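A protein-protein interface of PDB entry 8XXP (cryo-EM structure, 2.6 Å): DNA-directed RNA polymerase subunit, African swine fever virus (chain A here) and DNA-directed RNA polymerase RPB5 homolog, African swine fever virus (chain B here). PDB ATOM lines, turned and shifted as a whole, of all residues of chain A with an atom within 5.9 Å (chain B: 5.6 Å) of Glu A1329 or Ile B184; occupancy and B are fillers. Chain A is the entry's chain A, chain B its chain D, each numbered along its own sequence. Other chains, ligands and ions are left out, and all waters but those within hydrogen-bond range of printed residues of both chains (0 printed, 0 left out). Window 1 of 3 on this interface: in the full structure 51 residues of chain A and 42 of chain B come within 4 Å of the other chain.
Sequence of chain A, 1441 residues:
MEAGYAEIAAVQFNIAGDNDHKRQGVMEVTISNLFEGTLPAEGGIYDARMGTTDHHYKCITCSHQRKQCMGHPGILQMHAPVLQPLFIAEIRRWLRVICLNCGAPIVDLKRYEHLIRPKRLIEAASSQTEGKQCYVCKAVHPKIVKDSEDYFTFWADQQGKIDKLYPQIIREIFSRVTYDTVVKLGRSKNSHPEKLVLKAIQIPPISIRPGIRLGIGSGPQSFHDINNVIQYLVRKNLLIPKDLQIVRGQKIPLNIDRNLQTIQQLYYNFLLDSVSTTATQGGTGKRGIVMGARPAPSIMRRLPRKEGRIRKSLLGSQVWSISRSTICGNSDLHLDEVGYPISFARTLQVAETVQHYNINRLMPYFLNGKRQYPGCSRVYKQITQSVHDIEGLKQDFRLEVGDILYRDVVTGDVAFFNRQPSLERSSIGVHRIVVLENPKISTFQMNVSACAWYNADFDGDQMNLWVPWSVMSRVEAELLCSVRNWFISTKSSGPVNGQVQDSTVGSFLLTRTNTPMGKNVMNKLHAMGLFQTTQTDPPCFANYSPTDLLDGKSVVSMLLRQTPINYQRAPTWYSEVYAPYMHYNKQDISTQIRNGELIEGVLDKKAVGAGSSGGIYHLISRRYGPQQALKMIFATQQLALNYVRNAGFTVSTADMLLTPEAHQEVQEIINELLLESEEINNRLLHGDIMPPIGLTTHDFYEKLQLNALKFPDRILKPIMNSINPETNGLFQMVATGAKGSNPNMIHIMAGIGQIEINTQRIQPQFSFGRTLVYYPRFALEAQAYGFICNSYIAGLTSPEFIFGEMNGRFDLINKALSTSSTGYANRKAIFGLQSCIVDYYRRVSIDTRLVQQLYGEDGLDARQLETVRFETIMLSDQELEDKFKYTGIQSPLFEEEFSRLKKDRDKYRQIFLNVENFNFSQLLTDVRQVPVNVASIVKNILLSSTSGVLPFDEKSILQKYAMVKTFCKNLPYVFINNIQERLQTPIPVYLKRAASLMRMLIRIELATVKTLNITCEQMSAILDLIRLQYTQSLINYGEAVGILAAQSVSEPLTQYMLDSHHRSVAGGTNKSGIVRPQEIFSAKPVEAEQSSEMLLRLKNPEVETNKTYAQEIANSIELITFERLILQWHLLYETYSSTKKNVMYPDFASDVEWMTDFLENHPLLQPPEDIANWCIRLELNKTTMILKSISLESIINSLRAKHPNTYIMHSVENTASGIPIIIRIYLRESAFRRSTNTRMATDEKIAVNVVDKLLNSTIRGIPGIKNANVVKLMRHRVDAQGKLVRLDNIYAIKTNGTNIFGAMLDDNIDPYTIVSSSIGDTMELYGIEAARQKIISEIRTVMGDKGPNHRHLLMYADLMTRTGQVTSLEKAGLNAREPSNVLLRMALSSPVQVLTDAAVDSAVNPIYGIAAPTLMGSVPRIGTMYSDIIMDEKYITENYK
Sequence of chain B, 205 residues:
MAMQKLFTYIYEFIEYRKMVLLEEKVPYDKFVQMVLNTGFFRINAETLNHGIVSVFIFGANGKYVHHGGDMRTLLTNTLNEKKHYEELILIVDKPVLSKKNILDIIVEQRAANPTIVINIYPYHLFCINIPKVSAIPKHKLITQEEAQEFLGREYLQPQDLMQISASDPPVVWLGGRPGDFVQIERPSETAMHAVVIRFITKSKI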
ATOM      1  N   TYR A1326       1.149 -11.413   8.398  1.00  0.00           N
ATOM      2  CA  TYR A1326       1.632 -12.762   8.653  1.00  0.00           C
ATOM      3  C   TYR A1326       0.913 -13.489   9.775  1.00  0.00           C
ATOM      4  O   TYR A1326       0.850 -14.717   9.745  1.00  0.00           O
ATOM      5  CB  TYR A1326       3.131 -12.733   8.964  1.00  0.00           C
ATOM      6  CG  TYR A1326       3.993 -12.317   7.800  1.00  0.00           C
ATOM      7  CD1 TYR A1326       3.583 -12.532   6.494  1.00  0.00           C
ATOM      8  CD2 TYR A1326       5.217 -11.713   8.007  1.00  0.00           C
ATOM      9  CE1 TYR A1326       4.367 -12.158   5.431  1.00  0.00           C
ATOM     10  CE2 TYR A1326       6.008 -11.332   6.951  1.00  0.00           C
ATOM     11  CZ  TYR A1326       5.578 -11.557   5.666  1.00  0.00           C
ATOM     12  OH  TYR A1326       6.376 -11.178   4.615  1.00  0.00           O
ATOM     13  N   GLY A1327       0.381 -12.786  10.761  1.00  0.00           N
ATOM     14  CA  GLY A1327      -0.343 -13.412  11.846  1.00  0.00           C
ATOM     15  C   GLY A1327       0.284 -13.117  13.193  1.00  0.00           C
ATOM     16  O   GLY A1327       1.254 -12.374  13.315  1.00  0.00           O
ATOM     17  N   ILE A1328      -0.310 -13.720  14.223  1.00  0.00           N
ATOM     18  CA  ILE A1328       0.112 -13.442  15.591  1.00  0.00           C
ATOM     19  C   ILE A1328       1.436 -14.126  15.904  1.00  0.00           C
ATOM     20  O   ILE A1328       2.273 -13.578  16.629  1.00  0.00           O
ATOM     21  CB  ILE A1328      -0.991 -13.840  16.589  1.00  0.00           C
ATOM     22  CG1 ILE A1328      -0.626 -13.359  17.989  1.00  0.00           C
ATOM     23  CG2 ILE A1328      -1.239 -15.330  16.576  1.00  0.00           C
ATOM     24  CD1 ILE A1328      -0.430 -11.877  18.072  1.00  0.00           C
ATOM     25  N   GLU A1329       1.650 -15.329  15.376  1.00  0.00           N
ATOM     26  CA  GLU A1329       2.881 -16.048  15.678  1.00  0.00           C
ATOM     27  C   GLU A1329       4.092 -15.352  15.078  1.00  0.00           C
ATOM     28  O   GLU A1329       5.162 -15.321  15.691  1.00  0.00           O
ATOM     29  CB  GLU A1329       2.777 -17.484  15.185  1.00  0.00           C
ATOM     30  CG  GLU A1329       1.936 -18.376  16.072  1.00  0.00           C
ATOM     31  CD  GLU A1329       2.607 -18.668  17.392  1.00  0.00           C
ATOM     32  OE1 GLU A1329       3.847 -18.800  17.413  1.00  0.00           O
ATOM     33  OE2 GLU A1329       1.902 -18.767  18.413  1.00  0.00           O
ATOM     34  N   ALA A1330       3.948 -14.793  13.878  1.00  0.00           N
ATOM     35  CA  ALA A1330       5.039 -14.024  13.295  1.00  0.00           C
ATOM     36  C   ALA A1330       5.201 -12.673  13.973  1.00  0.00           C
ATOM     37  O   ALA A1330       6.323 -12.172  14.086  1.00  0.00           O
ATOM     38  CB  ALA A1330       4.814 -13.841  11.801  1.00  0.00           C
ATOM     39  N   ALA A1331       4.099 -12.058  14.405  1.00  0.00           N
ATOM     40  CA  ALA A1331       4.198 -10.833  15.188  1.00  0.00           C
ATOM     41  C   ALA A1331       4.853 -11.100  16.533  1.00  0.00           C
ATOM     42  O   ALA A1331       5.577 -10.250  17.059  1.00  0.00           O
ATOM     43  CB  ALA A1331       2.818 -10.219  15.384  1.00  0.00           C
ATOM     44  N   ARG A1332       4.594 -12.271  17.110  1.00  0.00           N
ATOM     45  CA  ARG A1332       5.238 -12.647  18.361  1.00  0.00           C
ATOM     46  C   ARG A1332       6.742 -12.792  18.180  1.00  0.00           C
ATOM     47  O   ARG A1332       7.520 -12.380  19.045  1.00  0.00           O
ATOM     48  CB  ARG A1332       4.615 -13.937  18.887  1.00  0.00           C
ATOM     49  CG  ARG A1332       5.186 -14.441  20.185  1.00  0.00           C
ATOM     50  CD  ARG A1332       5.908 -15.733  19.963  1.00  0.00           C
ATOM     51  NE  ARG A1332       6.397 -16.302  21.208  1.00  0.00           N
ATOM     52  CZ  ARG A1332       7.349 -17.219  21.277  1.00  0.00           C
ATOM     53  NH1 ARG A1332       7.947 -17.675  20.191  1.00  0.00           N
ATOM     54  NH2 ARG A1332       7.711 -17.688  22.466  1.00  0.00           N
ATOM     55  N   GLN A1333       7.174 -13.377  17.063  1.00  0.00           N
ATOM     56  CA  GLN A1333       8.601 -13.451  16.777  1.00  0.00           C
ATOM     57  C   GLN A1333       9.180 -12.082  16.458  1.00  0.00           C
ATOM     58  O   GLN A1333      10.345 -11.815  16.766  1.00  0.00           O
ATOM     59  CB  GLN A1333       8.860 -14.409  15.619  1.00  0.00           C
ATOM     60  CG  GLN A1333       8.667 -15.860  15.961  1.00  0.00           C
ATOM     61  CD  GLN A1333       9.827 -16.428  16.736  1.00  0.00           C
ATOM     62  OE1 GLN A1333      10.840 -15.763  16.936  1.00  0.00           O
ATOM     63  NE2 GLN A1333       9.691 -17.669  17.177  1.00  0.00           N
ATOM     64  N   LYS A1334       8.390 -11.212  15.831  1.00  0.00           N
ATOM     65  CA  LYS A1334       8.849  -9.860  15.549  1.00  0.00           C
ATOM     66  C   LYS A1334       9.096  -9.083  16.831  1.00  0.00           C
ATOM     67  O   LYS A1334      10.055  -8.310  16.918  1.00  0.00           O
ATOM     68  CB  LYS A1334       7.827  -9.139  14.671  1.00  0.00           C
ATOM     69  CG  LYS A1334       8.294  -7.807  14.127  1.00  0.00           C
ATOM     70  CD  LYS A1334       9.590  -7.942  13.358  1.00  0.00           C
ATOM     71  CE  LYS A1334       9.458  -8.917  12.209  1.00  0.00           C
ATOM     72  NZ  LYS A1334      10.767  -9.177  11.572  1.00  0.00           N
ATOM     73  N   ALA B 135       8.786 -16.358   7.998  1.00  0.00           N
ATOM     74  CA  ALA B 135       8.485 -15.807   9.312  1.00  0.00           C
ATOM     75  C   ALA B 135       7.281 -16.457   9.973  1.00  0.00           C
ATOM     76  O   ALA B 135       7.035 -16.195  11.153  1.00  0.00           O
ATOM     77  CB  ALA B 135       8.259 -14.299   9.206  1.00  0.00           C
ATOM     78  N   PRO B 137       5.575 -19.657  11.497  1.00  0.00           N
ATOM     79  CA  PRO B 137       5.823 -21.036  11.921  1.00  0.00           C
ATOM     80  C   PRO B 137       4.726 -21.966  11.437  1.00  0.00           C
ATOM     81  O   PRO B 137       3.617 -21.551  11.104  1.00  0.00           O
ATOM     82  CB  PRO B 137       5.835 -20.941  13.448  1.00  0.00           C
ATOM     83  CG  PRO B 137       5.077 -19.722  13.757  1.00  0.00           C
ATOM     84  CD  PRO B 137       5.283 -18.771  12.632  1.00  0.00           C
ATOM     85  N   LYS B 138       5.053 -23.251  11.399  1.00  0.00           N
ATOM     86  CA  LYS B 138       4.148 -24.232  10.819  1.00  0.00           C
ATOM     87  C   LYS B 138       2.920 -24.411  11.700  1.00  0.00           C
ATOM     88  O   LYS B 138       3.024 -24.860  12.844  1.00  0.00           O
ATOM     89  CB  LYS B 138       4.865 -25.560  10.625  1.00  0.00           C
ATOM     90  CG  LYS B 138       5.106 -25.900   9.178  1.00  0.00           C
ATOM     91  CD  LYS B 138       5.806 -24.757   8.469  1.00  0.00           C
ATOM     92  CE  LYS B 138       6.051 -25.083   7.011  1.00  0.00           C
ATOM     93  NZ  LYS B 138       6.440 -23.881   6.234  1.00  0.00           N
ATOM     94  N   HIS B 139       1.760 -24.063  11.158  1.00  0.00           N
ATOM     95  CA  HIS B 139       0.479 -24.251  11.817  1.00  0.00           C
ATOM     96  C   HIS B 139      -0.153 -25.542  11.325  1.00  0.00           C
ATOM     97  O   HIS B 139       0.003 -25.915  10.160  1.00  0.00           O
ATOM     98  CB  HIS B 139      -0.464 -23.084  11.522  1.00  0.00           C
ATOM     99  CG  HIS B 139      -0.018 -21.775  12.090  1.00  0.00           C
ATOM    100  ND1 HIS B 139       1.240 -21.259  11.876  1.00  0.00           N
ATOM    101  CD2 HIS B 139      -0.673 -20.866  12.845  1.00  0.00           C
ATOM    102  CE1 HIS B 139       1.346 -20.096  12.490  1.00  0.00           C
ATOM    103  NE2 HIS B 139       0.198 -19.833  13.083  1.00  0.00           N
ATOM    104  N   LYS B 140      -0.868 -26.223  12.211  1.00  0.00           N
ATOM    105  CA  LYS B 140      -1.661 -27.369  11.800  1.00  0.00           C
ATOM    106  C   LYS B 140      -2.845 -27.513  12.738  1.00  0.00           C
ATOM    107  O   LYS B 140      -2.723 -27.292  13.944  1.00  0.00           O
ATOM    108  CB  LYS B 140      -0.832 -28.660  11.768  1.00  0.00           C
ATOM    109  CG  LYS B 140      -0.642 -29.358  13.090  1.00  0.00           C
ATOM    110  CD  LYS B 140       0.265 -30.557  12.926  1.00  0.00           C
ATOM    111  CE  LYS B 140       0.313 -31.411  14.178  1.00  0.00           C
ATOM    112  NZ  LYS B 140      -0.795 -32.402  14.223  1.00  0.00           N
ATOM    113  N   ILE B 164      -6.026 -17.563  19.188  1.00  0.00           N
ATOM    114  CA  ILE B 164      -5.666 -17.173  17.833  1.00  0.00           C
ATOM    115  C   ILE B 164      -6.944 -16.854  17.075  1.00  0.00           C
ATOM    116  O   ILE B 164      -7.979 -17.497  17.274  1.00  0.00           O
ATOM    117  CB  ILE B 164      -4.830 -18.262  17.127  1.00  0.00           C
ATOM    118  CG1 ILE B 164      -4.143 -17.687  15.892  1.00  0.00           C
ATOM    119  CG2 ILE B 164      -5.671 -19.468  16.782  1.00  0.00           C
ATOM    120  CD1 ILE B 164      -2.970 -18.482  15.440  1.00  0.00           C
ATOM    121  N   ASP B 168      -6.510 -15.125  11.224  1.00  0.00           N
ATOM    122  CA  ASP B 168      -5.064 -15.169  11.115  1.00  0.00           C
ATOM    123  C   ASP B 168      -4.683 -15.821   9.790  1.00  0.00           C
ATOM    124  O   ASP B 168      -5.270 -16.844   9.423  1.00  0.00           O
ATOM    125  CB  ASP B 168      -4.473 -15.951  12.283  1.00  0.00           C
ATOM    126  CG  ASP B 168      -3.215 -15.327  12.828  1.00  0.00           C
ATOM    127  OD1 ASP B 168      -3.301 -14.238  13.425  1.00  0.00           O
ATOM    128  OD2 ASP B 168      -2.140 -15.940  12.679  1.00  0.00           O
ATOM    129  N   VAL B 182      -5.333 -25.162  16.927  1.00  0.00           N
ATOM    130  CA  VAL B 182      -4.242 -25.178  15.965  1.00  0.00           C
ATOM    131  C   VAL B 182      -2.935 -25.323  16.726  1.00  0.00           C
ATOM    132  O   VAL B 182      -2.652 -24.546  17.643  1.00  0.00           O
ATOM    133  CB  VAL B 182      -4.242 -23.917  15.082  1.00  0.00           C
ATOM    134  CG1 VAL B 182      -4.413 -22.682  15.917  1.00  0.00           C
ATOM    135  CG2 VAL B 182      -2.968 -23.838  14.283  1.00  0.00           C
ATOM    136  N   GLN B 183      -2.148 -26.322  16.352  1.00  0.00           N
ATOM    137  CA  GLN B 183      -0.842 -26.556  16.945  1.00  0.00           C
ATOM    138  C   GLN B 183       0.213 -25.867  16.097  1.00  0.00           C
ATOM    139  O   GLN B 183       0.231 -26.022  14.875  1.00  0.00           O
ATOM    140  CB  GLN B 183      -0.551 -28.050  17.046  1.00  0.00           C
ATOM    141  CG  GLN B 183       0.839 -28.372  17.520  1.00  0.00           C
ATOM    142  CD  GLN B 183       1.074 -29.854  17.647  1.00  0.00           C
ATOM    143  OE1 GLN B 183       0.329 -30.553  18.326  1.00  0.00           O
ATOM    144  NE2 GLN B 183       2.110 -30.347  16.989  1.00  0.00           N
ATOM    145  N   ILE B 184       1.083 -25.101  16.744  1.00  0.00           N
ATOM    146  CA  ILE B 184       2.113 -24.326  16.068  1.00  0.00           C
ATOM    147  C   ILE B 184       3.470 -24.866  16.487  1.00  0.00           C
ATOM    148  O   ILE B 184       3.728 -25.040  17.680  1.00  0.00           O
ATOM    149  CB  ILE B 184       1.999 -22.826  16.393  1.00  0.00           C
ATOM    150  CG1 ILE B 184       0.720 -22.244  15.800  1.00  0.00           C
ATOM    151  CG2 ILE B 184       3.201 -22.074  15.864  1.00  0.00           C
ATOM    152  CD1 ILE B 184      -0.353 -21.990  16.801  1.00  0.00           C
ATOM    153  N   GLU B 185       4.326 -25.144  15.506  1.00  0.00           N
ATOM    154  CA  GLU B 185       5.715 -25.530  15.748  1.00  0.00           C
ATOM    155  C   GLU B 185       6.573 -24.286  15.578  1.00  0.00           C
ATOM    156  O   GLU B 185       7.008 -23.958  14.477  1.00  0.00           O
ATOM    157  CB  GLU B 185       6.153 -26.641  14.805  1.00  0.00           C
ATOM    158  CG  GLU B 185       5.863 -28.035  15.311  1.00  0.00           C
ATOM    159  CD  GLU B 185       7.071 -28.676  15.963  1.00  0.00           C
ATOM    160  OE1 GLU B 185       8.016 -27.943  16.318  1.00  0.00           O
ATOM    161  OE2 GLU B 185       7.076 -29.915  16.119  1.00  0.00           O
ATOM    162  N   ARG B 186       6.825 -23.602  16.667  1.00  0.00           N
ATOM    163  CA  ARG B 186       7.538 -22.342  16.536  1.00  0.00           C
ATOM    164  C   ARG B 186       9.027 -22.548  16.731  1.00  0.00           C
ATOM    165  O   ARG B 186       9.428 -23.298  17.627  1.00  0.00           O
ATOM    166  CB  ARG B 186       7.017 -21.325  17.546  1.00  0.00           C
ATOM    167  CG  ARG B 186       6.583 -21.921  18.855  1.00  0.00           C
ATOM    168  CD  ARG B 186       6.379 -20.847  19.900  1.00  0.00           C
ATOM    169  NE  ARG B 186       5.088 -20.191  19.746  1.00  0.00           N
ATOM    170  CZ  ARG B 186       4.440 -19.574  20.724  1.00  0.00           C
ATOM    171  NH1 ARG B 186       4.940 -19.499  21.943  1.00  0.00           N
ATOM    172  NH2 ARG B 186       3.261 -19.019  20.469  1.00  0.00           N
ATOM    173  N   ALA B 194       9.770 -25.291  19.365  1.00  0.00           N
ATOM    174  CA  ALA B 194       8.818 -25.489  20.447  1.00  0.00           C
ATOM    175  C   ALA B 194       7.436 -25.698  19.852  1.00  0.00           C
ATOM    176  O   ALA B 194       7.190 -25.383  18.687  1.00  0.00           O
ATOM    177  CB  ALA B 194       8.801 -24.302  21.413  1.00  0.00           C
ATOM    178  N   VAL B 195       6.532 -26.235  20.664  1.00  0.00           N
ATOM    179  CA  VAL B 195       5.178 -26.560  20.237  1.00  0.00           C
ATOM    180  C   VAL B 195       4.195 -25.911  21.198  1.00  0.00           C
ATOM    181  O   VAL B 195       4.306 -26.082  22.415  1.00  0.00           O
ATOM    182  CB  VAL B 195       4.945 -28.080  20.184  1.00  0.00           C
ATOM    183  CG1 VAL B 195       3.470 -28.386  20.154  1.00  0.00           C
ATOM    184  CG2 VAL B 195       5.611 -28.671  18.985  1.00  0.00           C
ATOM    185  N   VAL B 196       3.228 -25.177  20.652  1.00  0.00           N
ATOM    186  CA  VAL B 196       2.121 -24.640  21.427  1.00  0.00           C
ATOM    187  C   VAL B 196       0.827 -25.007  20.720  1.00  0.00           C
ATOM    188  O   VAL B 196       0.817 -25.397  19.552  1.00  0.00           O
ATOM    189  CB  VAL B 196       2.205 -23.112  21.625  1.00  0.00           C
ATOM    190  CG1 VAL B 196       3.495 -22.734  22.316  1.00  0.00           C
ATOM    191  CG2 VAL B 196       2.068 -22.396  20.302  1.00  0.00           C
ATOM    192  N   ILE B 197      -0.270 -24.908  21.457  1.00  0.00           N
ATOM    193  CA  ILE B 197      -1.607 -25.100  20.920  1.00  0.00           C
ATOM    194  C   ILE B 197      -2.410 -23.848  21.228  1.00  0.00           C
ATOM    195  O   ILE B 197      -2.479 -23.422  22.384  1.00  0.00           O
ATOM    196  CB  ILE B 197      -2.276 -26.355  21.507  1.00  0.00           C
ATOM    197  CG1 ILE B 197      -1.510 -27.603  21.069  1.00  0.00           C
ATOM    198  CG2 ILE B 197      -3.722 -26.442  21.073  1.00  0.00           C
ATOM    199  CD1 ILE B 197      -1.909 -28.853  21.792  1.00  0.00           C
ATOM    200  N   ARG B 198      -2.997 -23.253  20.197  1.00  0.00           N
ATOM    201  CA  ARG B 198      -3.748 -22.018  20.336  1.00  0.00           C
ATOM    202  C   ARG B 198      -5.208 -22.254  19.989  1.00  0.00           C
ATOM    203  O   ARG B 198      -5.522 -22.949  19.022  1.00  0.00           O
ATOM    204  CB  ARG B 198      -3.171 -20.920  19.451  1.00  0.00           C
ATOM    205  CG  ARG B 198      -1.769 -20.523  19.827  1.00  0.00           C
ATOM    206  CD  ARG B 198      -1.356 -19.267  19.124  1.00  0.00           C
ATOM    207  NE  ARG B 198      -1.870 -18.083  19.793  1.00  0.00           N
ATOM    208  CZ  ARG B 198      -1.119 -17.079  20.220  1.00  0.00           C
ATOM    209  NH1 ARG B 198       0.193 -17.087  20.072  1.00  0.00           N
ATOM    210  NH2 ARG B 198      -1.701 -16.041  20.806  1.00  0.00           N
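The guanidinium group of Arg A1332 sits close to the side-chain amide nitrogen of Gln A1333, 3.5 Å away.
The backbone NH (N) of Ile B184 sits at hydrogen-bond distance from the backbone carbonyl oxygen (O) of Val B196 (2.8 Å).
The backbone carbonyl oxygen (O) of Pro B137 is in hydrogen-bond range of a ring nitrogen (ND1) of His B139 (2.5 Å).
The backbone carbonyl oxygen (O) of Arg B186 is in hydrogen-bond range of the backbone NH (N) of Ala B194.
The backbone carbonyl oxygen (O) of Val B182 lies within hydrogen-bond range of the backbone NH (N) of Arg B198 (2.9 Å).
The backbone NH (N) of Ile A1328 sits at hydrogen-bond distance from the side-chain carboxylate (OD1) of Asp B168, at 3.1 Å.
The side-chain carboxylate (OE2) of Glu A1329 is in salt-bridge range of the guanidinium group (NH1) of Arg B198, at 2.9 Å.
The guanidinium group of Arg B186 lies within salt-bridge range of the side-chain carboxylate of Glu A1329.
NH2 of Arg A1332 sits close to NH1 of Arg B186, at 3.4 Å.
Asp B168 touches Gly A1327 (OD2 to CA, 3.2 Å).
Ile A1328 touches Ile B164 (CG2 to CD1, 3.8 Å).
Glu A1329 touches Pro B137.
His B139 touches Glu A1329.
Glu A1329 touches Ile B184 (OE1 to CG2, 3.7 Å).
Ala A1330 touches Ala B135.
Of the 9 printed residues of chain A, 5 touch a printed residue of chain B.
Among the printed residues, 10 pairs touch across the chains.
Among the printed residues, Asp or Glu carboxylates within 4 Å of a Lys or Arg side-chain nitrogen of the other chain: Glu A1329 with Arg B186 and Glu A1329 with Arg B198.
Glu A1329 touches just these residues of chain B: Pro B137 (3.5 Å), His B139 (3.8 Å), Ile B184 (3.7 Å), Arg B186 (2.5 Å) and Arg B198 (2.9 Å).
Of chain A, only Glu A1329 comes within 4 Å of Ile B184.
Of the printed residues of chain A, Arg B186 touches Glu A1329 and Arg A1332.
Of the printed residues of chain A, Pro B137 touches Glu A1329.
Printed residues of chain A within 4 Å of Asp B168: Gly A1327 and Ile A1328.
Printed residues of chain B within 4 Å of Ala A1330: Ala B135.
Of the printed residues of chain B, Arg A1332 touches Arg B186.
Lys B140 touches none of the printed residues of chain A.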
